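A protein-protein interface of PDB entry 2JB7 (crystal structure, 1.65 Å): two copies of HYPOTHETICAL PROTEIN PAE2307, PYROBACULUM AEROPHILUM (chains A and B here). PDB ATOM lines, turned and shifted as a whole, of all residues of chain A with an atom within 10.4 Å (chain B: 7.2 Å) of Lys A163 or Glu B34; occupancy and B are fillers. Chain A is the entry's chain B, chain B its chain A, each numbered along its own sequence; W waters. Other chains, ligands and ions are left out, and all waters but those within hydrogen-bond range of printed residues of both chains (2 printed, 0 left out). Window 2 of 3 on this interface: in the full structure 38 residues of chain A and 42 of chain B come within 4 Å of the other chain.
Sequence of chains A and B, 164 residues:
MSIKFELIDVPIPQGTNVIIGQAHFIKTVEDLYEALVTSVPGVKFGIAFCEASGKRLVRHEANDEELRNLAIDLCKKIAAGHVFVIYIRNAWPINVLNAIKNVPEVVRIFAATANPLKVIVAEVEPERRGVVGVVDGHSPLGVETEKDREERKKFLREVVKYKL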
ATOM      1  N   ILE A  94      -9.739 -26.751  20.021  1.00  0.00           N
ATOM      2  CA  ILE A  94     -11.129 -27.266  19.916  1.00  0.00           C
ATOM      3  C   ILE A  94     -11.302 -28.679  20.480  1.00  0.00           C
ATOM      4  O   ILE A  94     -12.441 -29.068  20.777  1.00  0.00           O
ATOM      5  CB  ILE A  94     -11.731 -27.222  18.485  1.00  0.00           C
ATOM      6  CG1 ILE A  94     -10.896 -28.003  17.444  1.00  0.00           C
ATOM      7  CG2 ILE A  94     -11.956 -25.765  18.048  1.00  0.00           C
ATOM      8  CD1 ILE A  94     -11.608 -28.134  16.061  1.00  0.00           C
ATOM      9  N   ARG A 149     -15.760 -16.904   0.586  1.00  0.00           N
ATOM     10  CA  ARG A 149     -16.609 -17.866   1.347  1.00  0.00           C
ATOM     11  C   ARG A 149     -16.551 -19.302   0.756  1.00  0.00           C
ATOM     12  O   ARG A 149     -16.437 -20.298   1.467  1.00  0.00           O
ATOM     13  CB  ARG A 149     -18.042 -17.345   1.404  1.00  0.00           C
ATOM     14  CG  ARG A 149     -19.007 -18.314   2.085  1.00  0.00           C
ATOM     15  CD  ARG A 149     -20.313 -17.667   2.147  1.00  0.00           C
ATOM     16  NE  ARG A 149     -21.331 -18.487   2.784  1.00  0.00           N
ATOM     17  CZ  ARG A 149     -22.166 -19.296   2.154  1.00  0.00           C
ATOM     18  NH1 ARG A 149     -22.155 -19.436   0.822  1.00  0.00           N
ATOM     19  NH2 ARG A 149     -23.033 -19.967   2.890  1.00  0.00           N
ATOM     20  N   GLU A 151     -14.022 -20.549  -0.785  1.00  0.00           N
ATOM     21  CA  GLU A 151     -12.721 -21.112  -0.424  1.00  0.00           C
ATOM     22  C   GLU A 151     -12.709 -21.556   1.049  1.00  0.00           C
ATOM     23  O   GLU A 151     -12.153 -22.584   1.343  1.00  0.00           O
ATOM     24  CB  GLU A 151     -11.516 -20.221  -0.729  1.00  0.00           C
ATOM     25  CG  GLU A 151     -11.512 -18.826  -0.235  1.00  0.00           C
ATOM     26  CD  GLU A 151     -10.130 -18.101  -0.444  1.00  0.00           C
ATOM     27  OE1 GLU A 151      -9.147 -18.782  -0.883  1.00  0.00           O
ATOM     28  OE2 GLU A 151     -10.064 -16.864  -0.170  1.00  0.00           O
ATOM     29  N   ARG A 152     -13.316 -20.781   1.937  1.00  0.00           N
ATOM     30  CA  ARG A 152     -13.392 -21.157   3.368  1.00  0.00           C
ATOM     31  C   ARG A 152     -14.173 -22.470   3.546  1.00  0.00           C
ATOM     32  O   ARG A 152     -13.773 -23.377   4.314  1.00  0.00           O
ATOM     33  CB  ARG A 152     -14.054 -20.060   4.228  1.00  0.00           C
ATOM     34  CG  ARG A 152     -15.082 -20.651   5.232  1.00  0.00           C
ATOM     35  CD  ARG A 152     -15.552 -19.717   6.222  1.00  0.00           C
ATOM     36  NE  ARG A 152     -16.527 -18.716   5.816  1.00  0.00           N
ATOM     37  CZ  ARG A 152     -17.845 -18.882   5.760  1.00  0.00           C
ATOM     38  NH1 ARG A 152     -18.437 -20.072   5.924  1.00  0.00           N
ATOM     39  NH2 ARG A 152     -18.561 -17.803   5.508  1.00  0.00           N
ATOM     40  N   LYS A 153     -15.282 -22.567   2.829  1.00  0.00           N
ATOM     41  CA  LYS A 153     -16.123 -23.764   2.883  1.00  0.00           C
ATOM     42  C   LYS A 153     -15.363 -24.973   2.391  1.00  0.00           C
ATOM     43  O   LYS A 153     -15.450 -26.051   2.965  1.00  0.00           O
ATOM     44  CB  LYS A 153     -17.405 -23.558   2.068  1.00  0.00           C
ATOM     45  CG  LYS A 153     -18.429 -22.663   2.744  1.00  0.00           C
ATOM     46  CD  LYS A 153     -19.654 -22.286   1.881  1.00  0.00           C
ATOM     47  CE  LYS A 153     -20.003 -23.333   0.851  1.00  0.00           C
ATOM     48  NZ  LYS A 153     -21.156 -22.885  -0.024  1.00  0.00           N
ATOM     49  N   LYS A 154     -14.632 -24.820   1.274  1.00  0.00           N
ATOM     50  CA  LYS A 154     -13.825 -25.884   0.739  1.00  0.00           C
ATOM     51  C   LYS A 154     -12.752 -26.333   1.715  1.00  0.00           C
ATOM     52  O   LYS A 154     -12.517 -27.531   1.853  1.00  0.00           O
ATOM     53  CB  LYS A 154     -13.178 -25.399  -0.571  1.00  0.00           C
ATOM     54  CG  LYS A 154     -12.675 -26.463  -1.475  1.00  0.00           C
ATOM     55  CD  LYS A 154     -12.662 -25.901  -2.924  1.00  0.00           C
ATOM     56  CE  LYS A 154     -12.507 -27.008  -3.945  1.00  0.00           C
ATOM     57  NZ  LYS A 154     -11.213 -27.692  -3.709  1.00  0.00           N
ATOM     58  N   PHE A 155     -12.105 -25.386   2.375  1.00  0.00           N
ATOM     59  CA  PHE A 155     -11.074 -25.689   3.345  1.00  0.00           C
ATOM     60  C   PHE A 155     -11.672 -26.552   4.414  1.00  0.00           C
ATOM     61  O   PHE A 155     -11.109 -27.577   4.748  1.00  0.00           O
ATOM     62  CB  PHE A 155     -10.513 -24.430   3.988  1.00  0.00           C
ATOM     63  CG  PHE A 155      -9.630 -24.674   5.197  1.00  0.00           C
ATOM     64  CD1 PHE A 155      -8.341 -25.189   5.061  1.00  0.00           C
ATOM     65  CD2 PHE A 155     -10.074 -24.331   6.476  1.00  0.00           C
ATOM     66  CE1 PHE A 155      -7.513 -25.390   6.181  1.00  0.00           C
ATOM     67  CE2 PHE A 155      -9.267 -24.517   7.585  1.00  0.00           C
ATOM     68  CZ  PHE A 155      -7.983 -25.047   7.444  1.00  0.00           C
ATOM     69  N   LEU A 156     -12.834 -26.153   4.930  1.00  0.00           N
ATOM     70  CA  LEU A 156     -13.429 -26.973   6.023  1.00  0.00           C
ATOM     71  C   LEU A 156     -13.903 -28.344   5.610  1.00  0.00           C
ATOM     72  O   LEU A 156     -13.959 -29.225   6.429  1.00  0.00           O
ATOM     73  CB  LEU A 156     -14.561 -26.227   6.721  1.00  0.00           C
ATOM     74  CG  LEU A 156     -14.124 -24.959   7.453  1.00  0.00           C
ATOM     75  CD1 LEU A 156     -15.350 -24.198   7.996  1.00  0.00           C
ATOM     76  CD2 LEU A 156     -13.138 -25.230   8.595  1.00  0.00           C
ATOM     77  N   ARG A 157     -14.224 -28.527   4.340  1.00  0.00           N
ATOM     78  CA  ARG A 157     -14.780 -29.796   3.859  1.00  0.00           C
ATOM     79  C   ARG A 157     -13.745 -30.737   3.237  1.00  0.00           C
ATOM     80  O   ARG A 157     -13.814 -31.963   3.424  1.00  0.00           O
ATOM     81  CB  ARG A 157     -15.879 -29.451   2.869  1.00  0.00           C
ATOM     82  CG  ARG A 157     -17.132 -28.847   3.555  1.00  0.00           C
ATOM     83  CD  ARG A 157     -18.023 -27.949   2.727  1.00  0.00           C
ATOM     84  NE  ARG A 157     -19.131 -27.560   3.601  1.00  0.00           N
ATOM     85  CZ  ARG A 157     -19.049 -26.624   4.542  1.00  0.00           C
ATOM     86  NH1 ARG A 157     -17.960 -25.893   4.666  1.00  0.00           N
ATOM     87  NH2 ARG A 157     -20.081 -26.425   5.352  1.00  0.00           N
ATOM     88  N   GLU A 158     -12.806 -30.164   2.486  1.00  0.00           N
ATOM     89  CA  GLU A 158     -11.850 -30.955   1.730  1.00  0.00           C
ATOM     90  C   GLU A 158     -10.490 -31.054   2.387  1.00  0.00           C
ATOM     91  O   GLU A 158      -9.783 -32.051   2.159  1.00  0.00           O
ATOM     92  CB  GLU A 158     -11.698 -30.385   0.322  1.00  0.00           C
ATOM     93  CG  GLU A 158     -13.010 -30.461  -0.444  1.00  0.00           C
ATOM     94  CD  GLU A 158     -12.897 -30.123  -1.904  1.00  0.00           C
ATOM     95  OE1 GLU A 158     -11.764 -29.930  -2.404  1.00  0.00           O
ATOM     96  OE2 GLU A 158     -13.972 -30.051  -2.543  1.00  0.00           O
ATOM     97  N   VAL A 159     -10.088 -30.045   3.165  1.00  0.00           N
ATOM     98  CA  VAL A 159      -8.767 -30.074   3.779  1.00  0.00           C
ATOM     99  C   VAL A 159      -8.797 -30.621   5.182  1.00  0.00           C
ATOM    100  O   VAL A 159      -8.209 -31.663   5.444  1.00  0.00           O
ATOM    101  CB  VAL A 159      -8.082 -28.720   3.728  1.00  0.00           C
ATOM    102  CG1 VAL A 159      -6.696 -28.797   4.363  1.00  0.00           C
ATOM    103  CG2 VAL A 159      -7.978 -28.284   2.263  1.00  0.00           C
ATOM    104  N   VAL A 160      -9.476 -29.936   6.098  1.00  0.00           N
ATOM    105  CA  VAL A 160      -9.518 -30.425   7.472  1.00  0.00           C
ATOM    106  C   VAL A 160     -10.678 -31.390   7.753  1.00  0.00           C
ATOM    107  O   VAL A 160     -10.685 -32.029   8.798  1.00  0.00           O
ATOM    108  CB  VAL A 160      -9.516 -29.283   8.504  1.00  0.00           C
ATOM    109  CG1 VAL A 160      -8.156 -28.577   8.502  1.00  0.00           C
ATOM    110  CG2 VAL A 160     -10.656 -28.276   8.266  1.00  0.00           C
ATOM    111  N   LYS A 161     -11.660 -31.447   6.850  1.00  0.00           N
ATOM    112  CA  LYS A 161     -12.753 -32.419   6.869  1.00  0.00           C
ATOM    113  C   LYS A 161     -13.601 -32.303   8.125  1.00  0.00           C
ATOM    114  O   LYS A 161     -14.108 -33.318   8.608  1.00  0.00           O
ATOM    115  CB  LYS A 161     -12.228 -33.858   6.727  1.00  0.00           C
ATOM    116  N   TYR A 162     -13.716 -31.084   8.649  1.00  0.00           N
ATOM    117  CA  TYR A 162     -14.565 -30.836   9.834  1.00  0.00           C
ATOM    118  C   TYR A 162     -16.034 -30.584   9.497  1.00  0.00           C
ATOM    119  O   TYR A 162     -16.900 -30.586  10.389  1.00  0.00           O
ATOM    120  CB  TYR A 162     -14.052 -29.609  10.584  1.00  0.00           C
ATOM    121  CG  TYR A 162     -12.743 -29.803  11.307  1.00  0.00           C
ATOM    122  CD1 TYR A 162     -12.304 -31.059  11.741  1.00  0.00           C
ATOM    123  CD2 TYR A 162     -11.963 -28.702  11.622  1.00  0.00           C
ATOM    124  CE1 TYR A 162     -11.088 -31.174  12.421  1.00  0.00           C
ATOM    125  CE2 TYR A 162     -10.753 -28.820  12.286  1.00  0.00           C
ATOM    126  CZ  TYR A 162     -10.340 -30.039  12.710  1.00  0.00           C
ATOM    127  OH  TYR A 162      -9.147 -30.154  13.407  1.00  0.00           O
ATOM    128  N   LYS A 163     -16.318 -30.328   8.220  1.00  0.00           N
ATOM    129  CA  LYS A 163     -17.672 -30.143   7.729  1.00  0.00           C
ATOM    130  C   LYS A 163     -17.857 -31.052   6.518  1.00  0.00           C
ATOM    131  O   LYS A 163     -16.877 -31.452   5.892  1.00  0.00           O
ATOM    132  CB  LYS A 163     -17.925 -28.688   7.367  1.00  0.00           C
ATOM    133  CG  LYS A 163     -17.913 -27.722   8.558  1.00  0.00           C
ATOM    134  CD  LYS A 163     -19.087 -27.931   9.528  1.00  0.00           C
ATOM    135  CE  LYS A 163     -19.120 -26.883  10.617  1.00  0.00           C
ATOM    136  NZ  LYS A 163     -20.158 -27.177  11.653  1.00  0.00           N
ATOM    137  N   LEU A 164     -19.128 -31.388   6.213  1.00  0.00           N
ATOM    138  CA  LEU A 164     -19.468 -32.136   5.001  1.00  0.00           C
ATOM    139  C   LEU A 164     -20.074 -31.227   3.952  1.00  0.00           C
ATOM    140  O   LEU A 164     -20.155 -31.657   2.803  1.00  0.00           O
ATOM    141  CB  LEU A 164     -20.454 -33.247   5.366  1.00  0.00           C
ATOM    142  CG  LEU A 164     -19.984 -34.181   6.463  1.00  0.00           C
ATOM    143  CD1 LEU A 164     -21.122 -34.931   7.126  1.00  0.00           C
ATOM    144  CD2 LEU A 164     -18.933 -35.120   5.898  1.00  0.00           C
ATOM    145  OXT LEU A 164     -20.532 -30.108   4.186  1.00  0.00           O
ATOM    146  N   LYS B  27     -13.575 -21.941  11.556  1.00  0.00           N
ATOM    147  CA  LYS B  27     -14.809 -22.699  11.652  1.00  0.00           C
ATOM    148  C   LYS B  27     -15.795 -22.029  12.591  1.00  0.00           C
ATOM    149  O   LYS B  27     -16.995 -22.339  12.580  1.00  0.00           O
ATOM    150  CB  LYS B  27     -14.492 -24.089  12.131  1.00  0.00           C
ATOM    151  CG  LYS B  27     -15.676 -25.108  12.043  1.00  0.00           C
ATOM    152  CD  LYS B  27     -15.225 -26.579  12.126  1.00  0.00           C
ATOM    153  CE  LYS B  27     -14.805 -27.039  13.502  1.00  0.00           C
ATOM    154  NZ  LYS B  27     -15.991 -27.340  14.374  1.00  0.00           N
ATOM    155  N   THR B  28     -15.308 -21.107  13.408  1.00  0.00           N
ATOM    156  CA  THR B  28     -16.204 -20.290  14.257  1.00  0.00           C
ATOM    157  C   THR B  28     -17.453 -19.811  13.514  1.00  0.00           C
ATOM    158  O   THR B  28     -18.566 -19.828  14.044  1.00  0.00           O
ATOM    159  CB  THR B  28     -15.466 -19.069  14.836  1.00  0.00           C
ATOM    160  OG1 THR B  28     -14.405 -19.494  15.715  1.00  0.00           O
ATOM    161  CG2 THR B  28     -16.434 -18.137  15.586  1.00  0.00           C
ATOM    162  N   VAL B  29     -17.270 -19.285  12.319  1.00  0.00           N
ATOM    163  CA  VAL B  29     -18.372 -18.657  11.624  1.00  0.00           C
ATOM    164  C   VAL B  29     -19.486 -19.673  11.308  1.00  0.00           C
ATOM    165  O   VAL B  29     -20.684 -19.366  11.475  1.00  0.00           O
ATOM    166  CB  VAL B  29     -17.874 -17.918  10.352  1.00  0.00           C
ATOM    167  CG1 VAL B  29     -17.271 -18.850   9.335  1.00  0.00           C
ATOM    168  CG2 VAL B  29     -19.008 -17.146   9.694  1.00  0.00           C
ATOM    169  N   GLU B  30     -19.107 -20.864  10.852  1.00  0.00           N
ATOM    170  CA  GLU B  30     -20.121 -21.893  10.559  1.00  0.00           C
ATOM    171  C   GLU B  30     -20.743 -22.427  11.834  1.00  0.00           C
ATOM    172  O   GLU B  30     -21.979 -22.659  11.874  1.00  0.00           O
ATOM    173  CB  GLU B  30     -19.561 -23.064   9.768  1.00  0.00           C
ATOM    174  CG  GLU B  30     -19.027 -22.580   8.411  1.00  0.00           C
ATOM    175  CD  GLU B  30     -19.008 -23.654   7.337  1.00  0.00           C
ATOM    176  OE1 GLU B  30     -19.645 -24.715   7.497  1.00  0.00           O
ATOM    177  OE2 GLU B  30     -18.358 -23.416   6.283  1.00  0.00           O
ATOM    178  N   ASP B  31     -19.924 -22.640  12.855  1.00  0.00           N
ATOM    179  CA  ASP B  31     -20.480 -23.228  14.107  1.00  0.00           C
ATOM    180  C   ASP B  31     -21.460 -22.257  14.785  1.00  0.00           C
ATOM    181  O   ASP B  31     -22.502 -22.681  15.310  1.00  0.00           O
ATOM    182  CB  ASP B  31     -19.379 -23.691  15.060  1.00  0.00           C
ATOM    183  CG  ASP B  31     -18.626 -24.912  14.570  1.00  0.00           C
ATOM    184  OD1 ASP B  31     -19.097 -25.630  13.652  1.00  0.00           O
ATOM    185  OD2 ASP B  31     -17.532 -25.194  15.133  1.00  0.00           O
ATOM    186  N   LEU B  32     -21.175 -20.928  14.762  1.00  0.00           N
ATOM    187  CA  LEU B  32     -22.089 -19.939  15.326  1.00  0.00           C
ATOM    188  C   LEU B  32     -23.372 -19.843  14.469  1.00  0.00           C
ATOM    189  O   LEU B  32     -24.474 -19.816  15.007  1.00  0.00           O
ATOM    190  CB  LEU B  32     -21.433 -18.528  15.484  1.00  0.00           C
ATOM    191  CG  LEU B  32     -20.341 -18.461  16.568  1.00  0.00           C
ATOM    192  CD1 LEU B  32     -19.742 -17.085  16.556  1.00  0.00           C
ATOM    193  CD2 LEU B  32     -20.908 -18.776  17.984  1.00  0.00           C
ATOM    194  N   TYR B  33     -23.244 -19.899  13.137  1.00  0.00           N
ATOM    195  CA  TYR B  33     -24.428 -19.964  12.249  1.00  0.00           C
ATOM    196  C   TYR B  33     -25.317 -21.107  12.709  1.00  0.00           C
ATOM    197  O   TYR B  33     -26.530 -20.952  12.889  1.00  0.00           O
ATOM    198  CB  TYR B  33     -23.997 -20.196  10.797  1.00  0.00           C
ATOM    199  CG  TYR B  33     -25.147 -20.489   9.868  1.00  0.00           C
ATOM    200  CD1 TYR B  33     -25.793 -19.470   9.204  1.00  0.00           C
ATOM    201  CD2 TYR B  33     -25.601 -21.783   9.673  1.00  0.00           C
ATOM    202  CE1 TYR B  33     -26.879 -19.737   8.354  1.00  0.00           C
ATOM    203  CE2 TYR B  33     -26.699 -22.047   8.855  1.00  0.00           C
ATOM    204  CZ  TYR B  33     -27.316 -21.039   8.188  1.00  0.00           C
ATOM    205  OH  TYR B  33     -28.393 -21.343   7.361  1.00  0.00           O
ATOM    206  N   GLU B  34     -24.718 -22.282  12.879  1.00  0.00           N
ATOM    207  CA  GLU B  34     -25.487 -23.456  13.277  1.00  0.00           C
ATOM    208  C   GLU B  34     -26.113 -23.325  14.647  1.00  0.00           C
ATOM    209  O   GLU B  34     -27.271 -23.701  14.827  1.00  0.00           O
ATOM    210  CB  GLU B  34     -24.608 -24.684  13.181  1.00  0.00           C
ATOM    211  CG  GLU B  34     -24.240 -25.015  11.748  1.00  0.00           C
ATOM    212  CD  GLU B  34     -23.473 -26.288  11.585  1.00  0.00           C
ATOM    213  OE1 GLU B  34     -23.715 -27.245  12.385  1.00  0.00           O
ATOM    214  OE2 GLU B  34     -22.636 -26.342  10.634  1.00  0.00           O
ATOM    215  N   ALA B  35     -25.371 -22.780  15.608  1.00  0.00           N
ATOM    216  CA  ALA B  35     -25.895 -22.626  16.957  1.00  0.00           C
ATOM    217  C   ALA B  35     -27.145 -21.744  16.919  1.00  0.00           C
ATOM    218  O   ALA B  35     -28.167 -21.993  17.598  1.00  0.00           O
ATOM    219  CB  ALA B  35     -24.805 -22.053  17.860  1.00  0.00           C
ATOM    220  N   LEU B  36     -27.111 -20.723  16.078  1.00  0.00           N
ATOM    221  CA  LEU B  36     -28.245 -19.813  16.017  1.00  0.00           C
ATOM    222  C   LEU B  36     -29.419 -20.457  15.285  1.00  0.00           C
ATOM    223  O   LEU B  36     -30.520 -20.487  15.802  1.00  0.00           O
ATOM    224  CB  LEU B  36     -27.831 -18.508  15.356  1.00  0.00           C
ATOM    225  CG  LEU B  36     -26.795 -17.686  16.091  1.00  0.00           C
ATOM    226  CD1 LEU B  36     -26.209 -16.608  15.203  1.00  0.00           C
ATOM    227  CD2 LEU B  36     -27.384 -17.094  17.343  1.00  0.00           C
ATOM    228  N   VAL B  37     -29.202 -20.979  14.073  1.00  0.00           N
ATOM    229  CA  VAL B  37     -30.365 -21.453  13.297  1.00  0.00           C
ATOM    230  C   VAL B  37     -31.033 -22.696  13.904  1.00  0.00           C
ATOM    231  O   VAL B  37     -32.241 -22.924  13.710  1.00  0.00           O
ATOM    232  CB  VAL B  37     -29.940 -21.651  11.815  1.00  0.00           C
ATOM    233  CG1 VAL B  37     -29.092 -22.910  11.650  1.00  0.00           C
ATOM    234  CG2 VAL B  37     -31.112 -21.578  10.856  1.00  0.00           C
ATOM    235  N   THR B  38     -30.301 -23.467  14.707  1.00  0.00           N
ATOM    236  CA  THR B  38     -30.854 -24.679  15.292  1.00  0.00           C
ATOM    237  C   THR B  38     -31.430 -24.433  16.677  1.00  0.00           C
ATOM    238  O   THR B  38     -31.896 -25.366  17.315  1.00  0.00           O
ATOM    239  CB  THR B  38     -29.827 -25.853  15.377  1.00  0.00           C
ATOM    240  OG1 THR B  38     -28.787 -25.531  16.285  1.00  0.00           O
ATOM    241  CG2 THR B  38     -29.227 -26.194  14.002  1.00  0.00           C
ATOM    242  N   SER B  39     -31.379 -23.196  17.149  1.00  0.00           N
ATOM    243  CA  SER B  39     -31.921 -22.848  18.466  1.00  0.00           C
ATOM    244  C   SER B  39     -33.365 -22.368  18.440  1.00  0.00           C
ATOM    245  O   SER B  39     -34.154 -22.730  19.348  1.00  0.00           O
ATOM    246  CB  SER B  39     -31.027 -21.796  19.144  1.00  0.00           C
ATOM    247  OG  SER B  39     -29.859 -22.421  19.656  1.00  0.00           O
ATOM    248  N   PHE B  45     -30.795 -13.382  11.856  1.00  0.00           N
ATOM    249  CA  PHE B  45     -29.490 -13.045  12.430  1.00  0.00           C
ATOM    250  C   PHE B  45     -28.454 -12.642  11.399  1.00  0.00           C
ATOM    251  O   PHE B  45     -28.544 -12.963  10.201  1.00  0.00           O
ATOM    252  CB  PHE B  45     -28.977 -14.228  13.244  1.00  0.00           C
ATOM    253  CG  PHE B  45     -28.771 -15.439  12.413  1.00  0.00           C
ATOM    254  CD1 PHE B  45     -29.843 -16.291  12.160  1.00  0.00           C
ATOM    255  CD2 PHE B  45     -27.563 -15.654  11.783  1.00  0.00           C
ATOM    256  CE1 PHE B  45     -29.698 -17.378  11.326  1.00  0.00           C
ATOM    257  CE2 PHE B  45     -27.371 -16.763  10.945  1.00  0.00           C
ATOM    258  CZ  PHE B  45     -28.461 -17.638  10.717  1.00  0.00           C
ATOM    259  N   ILE B  47     -24.112 -12.878  11.608  1.00  0.00           N
ATOM    260  CA  ILE B  47     -22.929 -13.188  12.418  1.00  0.00           C
ATOM    261  C   ILE B  47     -21.647 -12.882  11.635  1.00  0.00           C
ATOM    262  O   ILE B  47     -21.548 -13.183  10.451  1.00  0.00           O
ATOM    263  CB  ILE B  47     -22.959 -14.649  12.994  1.00  0.00           C
ATOM    264  CG1 ILE B  47     -21.676 -14.941  13.813  1.00  0.00           C
ATOM    265  CG2 ILE B  47     -23.108 -15.703  11.910  1.00  0.00           C
ATOM    266  CD1 ILE B  47     -20.527 -15.549  13.030  1.00  0.00           C
ATOM    267  N   ALA B  99     -25.917 -22.440  23.848  1.00  0.00           N
ATOM    268  CA  ALA B  99     -25.429 -23.073  22.626  1.00  0.00           C
ATOM    269  C   ALA B  99     -24.132 -22.400  22.189  1.00  0.00           C
ATOM    270  O   ALA B  99     -23.152 -23.047  21.812  1.00  0.00           O
ATOM    271  CB  ALA B  99     -26.490 -22.984  21.547  1.00  0.00           C
ATOM    272  N   VAL B 103     -19.985 -23.872  21.823  1.00  0.00           N
ATOM    273  CA  VAL B 103     -19.258 -24.015  20.571  1.00  0.00           C
ATOM    274  C   VAL B 103     -17.768 -24.119  20.927  1.00  0.00           C
ATOM    275  O   VAL B 103     -17.241 -23.251  21.657  1.00  0.00           O
ATOM    276  CB  VAL B 103     -19.502 -22.828  19.696  1.00  0.00           C
ATOM    277  CG1 VAL B 103     -18.466 -22.779  18.514  1.00  0.00           C
ATOM    278  CG2 VAL B 103     -20.953 -22.854  19.148  1.00  0.00           C
ATOM    279  N   GLU B 105     -15.000 -23.485  19.533  1.00  0.00           N
ATOM    280  CA  GLU B 105     -14.138 -22.355  19.173  1.00  0.00           C
ATOM    281  C   GLU B 105     -14.323 -21.172  20.110  1.00  0.00           C
ATOM    282  O   GLU B 105     -13.450 -20.310  20.215  1.00  0.00           O
ATOM    283  CB  GLU B 105     -14.410 -21.883  17.758  1.00  0.00           C
ATOM    284  CG  GLU B 105     -13.869 -22.770  16.669  1.00  0.00           C
ATOM    285  CD  GLU B 105     -14.881 -23.796  16.266  1.00  0.00           C
ATOM    286  OE1 GLU B 105     -16.101 -23.585  16.582  1.00  0.00           O
ATOM    287  OE2 GLU B 105     -14.499 -24.774  15.592  1.00  0.00           O
HETATM  288  O   HOH W   1     -17.460 -29.213  12.747  1.00  0.00           O
HETATM  289  O   HOH W   2     -22.094 -25.853   8.051  1.00  0.00           O
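OE2 of Glu B30 lies within salt-bridge range of NH1 of Arg A152.
The guanidinium group (NH2) of Arg A157 is in salt-bridge range of the side-chain carboxylate (OE1) of Glu B30, at 2.8 Å.
The side-chain carboxylate (OD1) of Asp B31 is in salt-bridge range of the side-chain amino group (NZ) of Lys A163.
OE2 of Glu B34 lies within salt-bridge range of NZ of Lys A163 (2.8 Å).
NZ of Lys B27 is in salt-bridge range of OD2 of Asp B31 (2.7 Å).
OE1 of Glu B105 lies close to OD2 of Asp B31, at 2.6 Å.
OG1 of Thr B38 is in hydrogen-bond range of O of Glu B34 (2.8 Å).
The backbone carbonyl oxygen (O) of Leu A156 sits at hydrogen-bond distance from the backbone NH (N) of Lys A161 (3.2 Å).
The backbone carbonyl oxygen (O) of Leu A156 is in hydrogen-bond range of the backbone NH (N) of Tyr A162, 2.9 Å away.
The chain-end carboxylate (OXT) of Leu A164 lies within salt-bridge range of the guanidinium group (NE) of Arg A157, at 3.0 Å.
Among the printed residues, merely in contact across the chains: Ile A94 with Glu B105 (3.7 Å), Arg A152 with Val B29 (3.6 Å), Lys A153 with Glu B30 (3.6 Å), Leu A156 with Lys B27 (3.95 Å), Leu A156 with Glu B30 (3.5 Å), Tyr A162 with Lys B27 (3.6 Å) and Lys A163 with Glu B30 (3.6 Å).
Of the printed residues of chain B, Arg A152 touches Val B29 (3.6 Å) and Glu B30 (3.4 Å).
Of the printed residues of chain B, Lys A153 touches Glu B30 (3.6 Å).
Printed residues of chain B within 4 Å of Arg A157: Glu B30.
Printed residues of chain B within 4 Å of Tyr A162: Lys B27 (3.6 Å).
Of chain B, only Glu B30, Asp B31 and Glu B34 come within 4 Å of Lys A163.
Asp B31 touches one residue of chain A.
Glu B34 touches just one residue of chain A: Lys A163.
No residue of chain A comes within 4 Å of Ala B35.
Val B37 touches none of the printed residues of chain A.
No residue of chain A comes within 4 Å of Thr B38.
Of the 16 printed residues of chain A, 7 touch a printed residue of chain B.
Hydrophobic or aromatic side chains of chain A within 4 Å of the printed part of chain B: Ile A94, Leu A156 and Tyr A162.
Along chain A the printed residues that touch a printed residue of chain B span positions 94 to 163.
Of the 18 printed residues of chain B, 6 touch a printed residue of chain A.
Hydrophobic or aromatic side chains of chain B that line the printed part of chain A: Val B29.
Among the printed residues, 11 pairs touch across the chains.
Among the printed residues, Asp or Glu carboxylates within 4 Å of a Lys or Arg side-chain nitrogen of the other chain: Arg A152 with Glu B30 (3.4 Å), Arg A157 with Glu B30 (2.8 Å), Lys A163 with Asp B31 (2.7 Å) and Lys A163 with Glu B34 (2.8 Å).
No position is printed for both chains.
Water W2 lies within hydrogen-bond range of the side-chain carboxylate of Glu B34 (2.7 Å), the side-chain carboxylate of Glu B30 (2.8 Å) and the guanidinium group of Arg A157 (3.4 Å).
Water W1 bridges the backbone carbonyl oxygen (O) of Tyr A162 (2.8 Å) and the side-chain amino group (NZ) of Lys B27 (2.9 Å).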
